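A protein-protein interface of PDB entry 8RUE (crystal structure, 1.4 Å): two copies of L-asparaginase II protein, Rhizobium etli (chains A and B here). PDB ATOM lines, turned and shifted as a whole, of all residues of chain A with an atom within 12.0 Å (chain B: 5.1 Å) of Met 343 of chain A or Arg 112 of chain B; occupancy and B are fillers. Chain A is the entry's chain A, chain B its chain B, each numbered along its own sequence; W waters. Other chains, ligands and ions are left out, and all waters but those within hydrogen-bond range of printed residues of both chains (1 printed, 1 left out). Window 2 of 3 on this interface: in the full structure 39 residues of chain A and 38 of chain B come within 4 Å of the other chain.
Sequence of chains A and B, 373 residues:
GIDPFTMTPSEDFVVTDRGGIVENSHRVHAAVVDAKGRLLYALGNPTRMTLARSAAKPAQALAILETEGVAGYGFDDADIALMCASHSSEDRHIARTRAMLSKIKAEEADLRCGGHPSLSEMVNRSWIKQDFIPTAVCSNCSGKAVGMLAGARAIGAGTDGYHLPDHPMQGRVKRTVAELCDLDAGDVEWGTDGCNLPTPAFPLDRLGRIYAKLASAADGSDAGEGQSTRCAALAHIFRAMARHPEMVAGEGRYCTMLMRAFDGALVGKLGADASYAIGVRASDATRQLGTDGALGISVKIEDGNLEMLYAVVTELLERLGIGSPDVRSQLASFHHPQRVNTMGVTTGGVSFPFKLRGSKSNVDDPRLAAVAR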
ATOM      1  N   ARG A  18     -28.885 -15.359 -15.787  1.00  0.00           N
ATOM      2  CA  ARG A  18     -27.609 -15.021 -15.189  1.00  0.00           C
ATOM      3  C   ARG A  18     -26.893 -14.211 -16.260  1.00  0.00           C
ATOM      4  O   ARG A  18     -26.531 -14.744 -17.321  1.00  0.00           O
ATOM      5  CB  ARG A  18     -26.840 -16.305 -14.859  1.00  0.00           C
ATOM      6  CG  ARG A  18     -25.501 -16.096 -14.086  1.00  0.00           C
ATOM      7  CD  ARG A  18     -24.956 -17.423 -13.560  1.00  0.00           C
ATOM      8  NE  ARG A  18     -25.832 -17.973 -12.538  1.00  0.00           N
ATOM      9  CZ  ARG A  18     -25.764 -17.667 -11.243  1.00  0.00           C
ATOM     10  NH1 ARG A  18     -24.783 -16.907 -10.750  1.00  0.00           N
ATOM     11  NH2 ARG A  18     -26.697 -18.136 -10.419  1.00  0.00           N
ATOM     12  N   GLN A 338     -33.922 -11.381  -4.949  1.00  0.00           N
ATOM     13  CA  GLN A 338     -32.521 -11.010  -5.042  1.00  0.00           C
ATOM     14  C   GLN A 338     -31.698 -12.093  -5.732  1.00  0.00           C
ATOM     15  O   GLN A 338     -31.916 -13.295  -5.542  1.00  0.00           O
ATOM     16  CB  GLN A 338     -31.946 -10.691  -3.664  1.00  0.00           C
ATOM     17  CG  GLN A 338     -32.041 -11.798  -2.635  1.00  0.00           C
ATOM     18  CD  GLN A 338     -31.295 -11.438  -1.348  1.00  0.00           C
ATOM     19  OE1 GLN A 338     -30.091 -11.152  -1.375  1.00  0.00           O
ATOM     20  NE2 GLN A 338     -32.010 -11.437  -0.218  1.00  0.00           N
ATOM     21  N   ARG A 339     -30.752 -11.642  -6.561  1.00  0.00           N
ATOM     22  CA  ARG A 339     -29.796 -12.514  -7.240  1.00  0.00           C
ATOM     23  C   ARG A 339     -28.401 -11.937  -7.014  1.00  0.00           C
ATOM     24  O   ARG A 339     -27.786 -11.391  -7.944  1.00  0.00           O
ATOM     25  CB  ARG A 339     -30.131 -12.628  -8.718  1.00  0.00           C
ATOM     26  CG  ARG A 339     -31.412 -13.411  -8.963  1.00  0.00           C
ATOM     27  CD  ARG A 339     -31.158 -14.870  -8.698  1.00  0.00           C
ATOM     28  NE  ARG A 339     -32.279 -15.727  -9.060  1.00  0.00           N
ATOM     29  CZ  ARG A 339     -33.236 -16.121  -8.223  1.00  0.00           C
ATOM     30  NH1 ARG A 339     -33.342 -15.624  -7.003  1.00  0.00           N
ATOM     31  NH2 ARG A 339     -34.111 -17.039  -8.622  1.00  0.00           N
ATOM     32  N   VAL A 340     -27.918 -12.064  -5.774  1.00  0.00           N
ATOM     33  CA  VAL A 340     -26.661 -11.472  -5.320  1.00  0.00           C
ATOM     34  C   VAL A 340     -25.753 -12.591  -4.839  1.00  0.00           C
ATOM     35  O   VAL A 340     -26.175 -13.445  -4.047  1.00  0.00           O
ATOM     36  CB  VAL A 340     -26.904 -10.448  -4.196  1.00  0.00           C
ATOM     37  CG1 VAL A 340     -25.588  -9.910  -3.656  1.00  0.00           C
ATOM     38  CG2 VAL A 340     -27.744  -9.290  -4.730  1.00  0.00           C
ATOM     39  N   ASN A 341     -24.514 -12.600  -5.329  1.00  0.00           N
ATOM     40  CA  ASN A 341     -23.630 -13.735  -5.098  1.00  0.00           C
ATOM     41  C   ASN A 341     -22.921 -13.591  -3.750  1.00  0.00           C
ATOM     42  O   ASN A 341     -23.191 -12.674  -2.967  1.00  0.00           O
ATOM     43  CB  ASN A 341     -22.729 -13.990  -6.310  1.00  0.00           C
ATOM     44  CG  ASN A 341     -21.615 -12.957  -6.476  1.00  0.00           C
ATOM     45  OD1 ASN A 341     -21.343 -12.127  -5.611  1.00  0.00           O
ATOM     46  ND2 ASN A 341     -20.922 -13.065  -7.579  1.00  0.00           N
ATOM     47  N   THR A 342     -21.986 -14.509  -3.473  1.00  0.00           N
ATOM     48  CA  THR A 342     -21.301 -14.527  -2.176  1.00  0.00           C
ATOM     49  C   THR A 342     -20.390 -13.321  -1.962  1.00  0.00           C
ATOM     50  O   THR A 342     -19.888 -13.140  -0.840  1.00  0.00           O
ATOM     51  CB  THR A 342     -20.478 -15.816  -1.988  1.00  0.00           C
ATOM     52  OG1 THR A 342     -19.419 -15.847  -2.965  1.00  0.00           O
ATOM     53  CG2 THR A 342     -21.376 -17.069  -2.132  1.00  0.00           C
ATOM     54  N   MET A 343     -20.142 -12.522  -3.002  1.00  0.00           N
ATOM     55  CA  MET A 343     -19.292 -11.339  -2.923  1.00  0.00           C
ATOM     56  C   MET A 343     -20.082 -10.046  -3.074  1.00  0.00           C
ATOM     57  O   MET A 343     -19.483  -8.969  -3.212  1.00  0.00           O
ATOM     58  CB  MET A 343     -18.140 -11.430  -3.939  1.00  0.00           C
ATOM     59  CG  MET A 343     -17.193 -12.588  -3.670  1.00  0.00           C
ATOM     60  SD  MET A 343     -16.403 -12.543  -2.045  1.00  0.00           S
ATOM     61  CE  MET A 343     -15.245 -11.180  -2.256  1.00  0.00           C
ATOM     62  N   GLY A 344     -21.413 -10.125  -3.030  1.00  0.00           N
ATOM     63  CA  GLY A 344     -22.278  -8.958  -3.056  1.00  0.00           C
ATOM     64  C   GLY A 344     -22.626  -8.455  -4.437  1.00  0.00           C
ATOM     65  O   GLY A 344     -23.169  -7.345  -4.564  1.00  0.00           O
ATOM     66  N   VAL A 345     -22.335  -9.228  -5.477  1.00  0.00           N
ATOM     67  CA  VAL A 345     -22.494  -8.783  -6.852  1.00  0.00           C
ATOM     68  C   VAL A 345     -23.809  -9.326  -7.393  1.00  0.00           C
ATOM     69  O   VAL A 345     -24.091 -10.517  -7.262  1.00  0.00           O
ATOM     70  CB  VAL A 345     -21.321  -9.287  -7.703  1.00  0.00           C
ATOM     71  CG1 VAL A 345     -21.550  -8.977  -9.179  1.00  0.00           C
ATOM     72  CG2 VAL A 345     -20.028  -8.669  -7.206  1.00  0.00           C
ATOM     73  N   THR A 346     -24.583  -8.475  -8.053  1.00  0.00           N
ATOM     74  CA  THR A 346     -25.813  -8.934  -8.699  1.00  0.00           C
ATOM     75  C   THR A 346     -25.472  -9.710  -9.961  1.00  0.00           C
ATOM     76  O   THR A 346     -24.839  -9.174 -10.884  1.00  0.00           O
ATOM     77  CB  THR A 346     -26.687  -7.742  -9.057  1.00  0.00           C
ATOM     78  OG1 THR A 346     -27.063  -7.032  -7.866  1.00  0.00           O
ATOM     79  CG2 THR A 346     -27.950  -8.213  -9.790  1.00  0.00           C
ATOM     80  N   THR A 347     -25.912 -10.972 -10.014  1.00  0.00           N
ATOM     81  CA  THR A 347     -25.558 -11.837 -11.121  1.00  0.00           C
ATOM     82  C   THR A 347     -26.698 -12.101 -12.085  1.00  0.00           C
ATOM     83  O   THR A 347     -26.463 -12.712 -13.131  1.00  0.00           O
ATOM     84  CB  THR A 347     -25.068 -13.205 -10.598  1.00  0.00           C
ATOM     85  OG1 THR A 347     -26.070 -13.774  -9.766  1.00  0.00           O
ATOM     86  CG2 THR A 347     -23.748 -13.105  -9.812  1.00  0.00           C
ATOM     87  N   GLY A 348     -27.923 -11.721 -11.749  1.00  0.00           N
ATOM     88  CA  GLY A 348     -29.023 -12.075 -12.617  1.00  0.00           C
ATOM     89  C   GLY A 348     -30.326 -11.477 -12.150  1.00  0.00           C
ATOM     90  O   GLY A 348     -30.343 -10.548 -11.341  1.00  0.00           O
ATOM     91  N   ALA B 109      -7.219 -14.359   2.822  1.00  0.00           N
ATOM     92  CA  ALA B 109      -7.581 -13.027   2.346  1.00  0.00           C
ATOM     93  C   ALA B 109      -7.288 -12.830   0.860  1.00  0.00           C
ATOM     94  O   ALA B 109      -7.811 -11.882   0.268  1.00  0.00           O
ATOM     95  CB  ALA B 109      -6.884 -11.954   3.177  1.00  0.00           C
ATOM     96  N   ASP B 110      -6.469 -13.701   0.242  1.00  0.00           N
ATOM     97  CA  ASP B 110      -6.188 -13.598  -1.181  1.00  0.00           C
ATOM     98  C   ASP B 110      -7.264 -14.224  -2.048  1.00  0.00           C
ATOM     99  O   ASP B 110      -7.274 -13.987  -3.266  1.00  0.00           O
ATOM    100  CB  ASP B 110      -4.846 -14.266  -1.507  1.00  0.00           C
ATOM    101  CG  ASP B 110      -3.676 -13.587  -0.804  1.00  0.00           C
ATOM    102  OD1 ASP B 110      -3.675 -12.330  -0.731  1.00  0.00           O
ATOM    103  OD2 ASP B 110      -2.744 -14.289  -0.335  1.00  0.00           O
ATOM    104  N   LEU B 111      -8.146 -15.034  -1.474  1.00  0.00           N
ATOM    105  CA  LEU B 111      -9.220 -15.591  -2.272  1.00  0.00           C
ATOM    106  C   LEU B 111     -10.260 -14.526  -2.573  1.00  0.00           C
ATOM    107  O   LEU B 111     -10.431 -13.541  -1.834  1.00  0.00           O
ATOM    108  CB  LEU B 111      -9.887 -16.753  -1.534  1.00  0.00           C
ATOM    109  CG  LEU B 111      -8.997 -17.957  -1.256  1.00  0.00           C
ATOM    110  CD1 LEU B 111      -9.771 -18.961  -0.388  1.00  0.00           C
ATOM    111  CD2 LEU B 111      -8.571 -18.608  -2.568  1.00  0.00           C
ATOM    112  N   ARG B 112     -10.965 -14.729  -3.678  1.00  0.00           N
ATOM    113  CA  ARG B 112     -11.922 -13.750  -4.170  1.00  0.00           C
ATOM    114  C   ARG B 112     -13.337 -14.332  -4.273  1.00  0.00           C
ATOM    115  O   ARG B 112     -14.193 -13.767  -4.958  1.00  0.00           O
ATOM    116  CB  ARG B 112     -11.425 -13.150  -5.496  1.00  0.00           C
ATOM    117  CG  ARG B 112     -10.140 -12.323  -5.371  1.00  0.00           C
ATOM    118  CD  ARG B 112     -10.394 -10.989  -4.653  1.00  0.00           C
ATOM    119  NE  ARG B 112      -9.168 -10.216  -4.409  1.00  0.00           N
ATOM    120  CZ  ARG B 112      -8.462 -10.289  -3.288  1.00  0.00           C
ATOM    121  NH1 ARG B 112      -8.830 -11.094  -2.300  1.00  0.00           N
ATOM    122  NH2 ARG B 112      -7.356  -9.549  -3.162  1.00  0.00           N
ATOM    123  N   CYS B 113     -13.594 -15.449  -3.591  1.00  0.00           N
ATOM    124  CA  CYS B 113     -14.904 -16.073  -3.444  1.00  0.00           C
ATOM    125  C   CYS B 113     -15.361 -15.899  -2.003  1.00  0.00           C
ATOM    126  O   CYS B 113     -14.550 -15.613  -1.120  1.00  0.00           O
ATOM    127  CB  CYS B 113     -14.830 -17.574  -3.798  1.00  0.00           C
ATOM    128  SG  CYS B 113     -13.575 -18.529  -2.830  1.00  0.00           S
ATOM    129  N   GLY B 114     -16.660 -16.089  -1.758  1.00  0.00           N
ATOM    130  CA  GLY B 114     -17.248 -15.877  -0.438  1.00  0.00           C
ATOM    131  C   GLY B 114     -17.868 -17.125   0.155  1.00  0.00           C
ATOM    132  O   GLY B 114     -18.155 -18.091  -0.570  1.00  0.00           O
ATOM    133  N   ASP B 160      -4.347  -9.925  -7.281  1.00  0.00           N
ATOM    134  CA  ASP B 160      -5.519  -9.254  -6.709  1.00  0.00           C
ATOM    135  C   ASP B 160      -6.795  -9.468  -7.529  1.00  0.00           C
ATOM    136  O   ASP B 160      -7.901  -9.551  -6.975  1.00  0.00           O
ATOM    137  CB  ASP B 160      -5.229  -7.759  -6.591  1.00  0.00           C
ATOM    138  CG  ASP B 160      -6.373  -6.998  -5.939  1.00  0.00           C
ATOM    139  OD1 ASP B 160      -6.756  -7.370  -4.808  1.00  0.00           O
ATOM    140  OD2 ASP B 160      -6.884  -6.031  -6.555  1.00  0.00           O
ATOM    141  N   TYR B 162      -7.388 -12.057  -9.909  1.00  0.00           N
ATOM    142  CA  TYR B 162      -7.298 -13.295 -10.675  1.00  0.00           C
ATOM    143  C   TYR B 162      -8.655 -13.752 -11.197  1.00  0.00           C
ATOM    144  O   TYR B 162      -8.698 -14.523 -12.156  1.00  0.00           O
ATOM    145  CB  TYR B 162      -6.712 -14.411  -9.792  1.00  0.00           C
ATOM    146  CG  TYR B 162      -7.642 -14.979  -8.712  1.00  0.00           C
ATOM    147  CD1 TYR B 162      -8.648 -15.909  -9.039  1.00  0.00           C
ATOM    148  CD2 TYR B 162      -7.486 -14.618  -7.387  1.00  0.00           C
ATOM    149  CE1 TYR B 162      -9.496 -16.431  -8.076  1.00  0.00           C
ATOM    150  CE2 TYR B 162      -8.329 -15.113  -6.410  1.00  0.00           C
ATOM    151  CZ  TYR B 162      -9.328 -16.019  -6.753  1.00  0.00           C
ATOM    152  OH  TYR B 162     -10.167 -16.515  -5.794  1.00  0.00           O
ATOM    153  N   HIS B 163      -9.747 -13.300 -10.586  1.00  0.00           N
ATOM    154  CA  HIS B 163     -11.087 -13.734 -10.950  1.00  0.00           C
ATOM    155  C   HIS B 163     -11.744 -12.846 -12.005  1.00  0.00           C
ATOM    156  O   HIS B 163     -12.850 -13.172 -12.462  1.00  0.00           O
ATOM    157  CB  HIS B 163     -11.967 -13.709  -9.702  1.00  0.00           C
ATOM    158  CG  HIS B 163     -12.085 -12.341  -9.102  1.00  0.00           C
ATOM    159  ND1 HIS B 163     -10.992 -11.588  -8.713  1.00  0.00           N
ATOM    160  CD2 HIS B 163     -13.175 -11.584  -8.841  1.00  0.00           C
ATOM    161  CE1 HIS B 163     -11.408 -10.426  -8.242  1.00  0.00           C
ATOM    162  NE2 HIS B 163     -12.729 -10.395  -8.311  1.00  0.00           N
ATOM    163  N   GLY B 194     -21.825 -17.895  -8.519  1.00  0.00           N
ATOM    164  CA  GLY B 194     -21.980 -17.567  -7.099  1.00  0.00           C
ATOM    165  C   GLY B 194     -20.684 -17.246  -6.384  1.00  0.00           C
ATOM    166  O   GLY B 194     -20.676 -16.483  -5.408  1.00  0.00           O
ATOM    167  N   CYS B 195     -19.574 -17.816  -6.855  1.00  0.00           N
ATOM    168  CA  CYS B 195     -18.260 -17.596  -6.271  1.00  0.00           C
ATOM    169  C   CYS B 195     -17.568 -16.363  -6.851  1.00  0.00           C
ATOM    170  O   CYS B 195     -16.427 -16.069  -6.463  1.00  0.00           O
ATOM    171  CB  CYS B 195     -17.396 -18.838  -6.524  1.00  0.00           C
ATOM    172  SG  CYS B 195     -17.097 -19.095  -8.306  1.00  0.00           S
ATOM    173  N   ASN B 196     -18.203 -15.663  -7.797  1.00  0.00           N
ATOM    174  CA  ASN B 196     -17.751 -14.390  -8.411  1.00  0.00           C
ATOM    175  C   ASN B 196     -16.741 -14.594  -9.540  1.00  0.00           C
ATOM    176  O   ASN B 196     -16.124 -13.609  -9.987  1.00  0.00           O
ATOM    177  CB  ASN B 196     -17.272 -13.348  -7.390  1.00  0.00           C
ATOM    178  CG  ASN B 196     -17.562 -11.922  -7.832  1.00  0.00           C
ATOM    179  OD1 ASN B 196     -18.554 -11.659  -8.502  1.00  0.00           O
ATOM    180  ND2 ASN B 196     -16.679 -10.995  -7.464  1.00  0.00           N
HETATM  181  O   HOH W   1     -18.291 -18.955  -3.262  1.00  0.00           O
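The side-chain amide nitrogen of Asn 341 of chain A lies within hydrogen-bond range of the side-chain amide oxygen of Asn 196 of chain B (2.9 Å).
The side-chain hydroxyl of Thr 342 of chain A is in hydrogen-bond range of the backbone NH of Gly 114 of chain B.
The side-chain hydroxyl of Thr 342 of chain A sits at hydrogen-bond distance from the backbone carbonyl oxygen of Gly 194 of chain B (2.8 Å).
The side-chain sulfur of Met 343 of chain A is in hydrogen-bond range of the backbone NH of Gly 114 of chain B (3.6 Å).
SD of Met 343 of chain A lies close to O of Cys 113 of chain B.
N of Met 343 of chain A is in hydrogen-bond range of OD1 of Asn 341 of chain A.
N of Gly 344 of chain A is in hydrogen-bond range of OD1 of Asn 341 of chain A (3.3 Å).
The side-chain amide oxygen of Asn 341 of chain A sits at hydrogen-bond distance from the backbone NH of Val 345 of chain A (3.1 Å).
NH1 of Arg 112 of chain B sits at hydrogen-bond distance from O of Ala 109 of chain B (2.9 Å).
The backbone carbonyl oxygen (O) of Asp 110 of chain B sits at hydrogen-bond distance from the guanidinium group (NH1) of Arg 112 of chain B.
The backbone NH (N) of Arg 112 of chain B lies within hydrogen-bond range of the side-chain hydroxyl (OH) of Tyr 162 of chain B.
Among the printed residues, merely in contact across the chains: Arg 18 of chain A with Gly 194 of chain B, Asn 341 of chain A with Gly 194 of chain B, Thr 342 of chain A with Cys 195 of chain B, Met 343 of chain A with Arg 112 of chain B, Met 343 of chain A with Asn 196 of chain B and Val 345 of chain A with Asn 196 of chain B.
Met 343 of chain A touches just these residues of chain B: Arg 112 (3.5 Å), Cys 113 (3.5 Å), Gly 114 (3.6 Å) and Asn 196 (3.8 Å).
Arg 112 of chain B touches one residue of chain A.
No residue of chain A comes within 4 Å of Ala 109 of chain B.
No residue of chain A comes within 4 Å of Asp 110 of chain B.
Leu 111 of chain B touches none of the printed residues of chain A.
Of chain A, only Met 343 comes within 4 Å of Cys 113 of chain B.
Gly 114 of chain B touches just these residues of chain A: Thr 342 and Met 343.
No residue of chain A comes within 4 Å of Tyr 162 of chain B.
No residue of chain A comes within 4 Å of His 163 of chain B.
Gly 194 of chain B touches three residues of chain A.
Cys 195 of chain B touches one residue of chain A.
Of chain A, only Asn 341 (2.9 Å), Met 343 (3.8 Å) and Val 345 (3.6 Å) come within 4 Å of Asn 196 of chain B.
Of the printed residues of chain B, Thr 342 of chain A touches Gly 114 (3.0 Å), Gly 194 (2.8 Å) and Cys 195 (3.9 Å).
Printed residues of chain B within 4 Å of Arg 18 of chain A: Gly 194.
Printed residues of chain B within 4 Å of Asn 341 of chain A: Gly 194 (3.4 Å) and Asn 196 (2.9 Å).
The nearest residue of chain B that does not touch Met 343 of chain A is Cys 195 of chain B (4.5 Å).
Of the 12 printed residues of chain A, 5 touch a printed residue of chain B.
Printed residues of chain A that touch a printed residue of chain B: Arg 18, Asn 341, Thr 342, Met 343 and Val 345.
Hydrophobic or aromatic side chains of chain A that line the printed part of chain B: Met 343 and Val 345.
Among the printed residues, no Asp or Glu carboxylate lies within 4 Å of a Lys or Arg side-chain nitrogen of the other chain.
No position is printed for both chains.
Of the 11 pairs that touch across the chains among the printed residues, none has its exchanged pair printed and touching as well.
Water W1 lies within hydrogen-bond range of the backbone carbonyl oxygen (O) of Gly 114 of chain B (2.8 Å) and the side-chain hydroxyl (OG1) of Thr 342 of chain A (3.3 Å).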
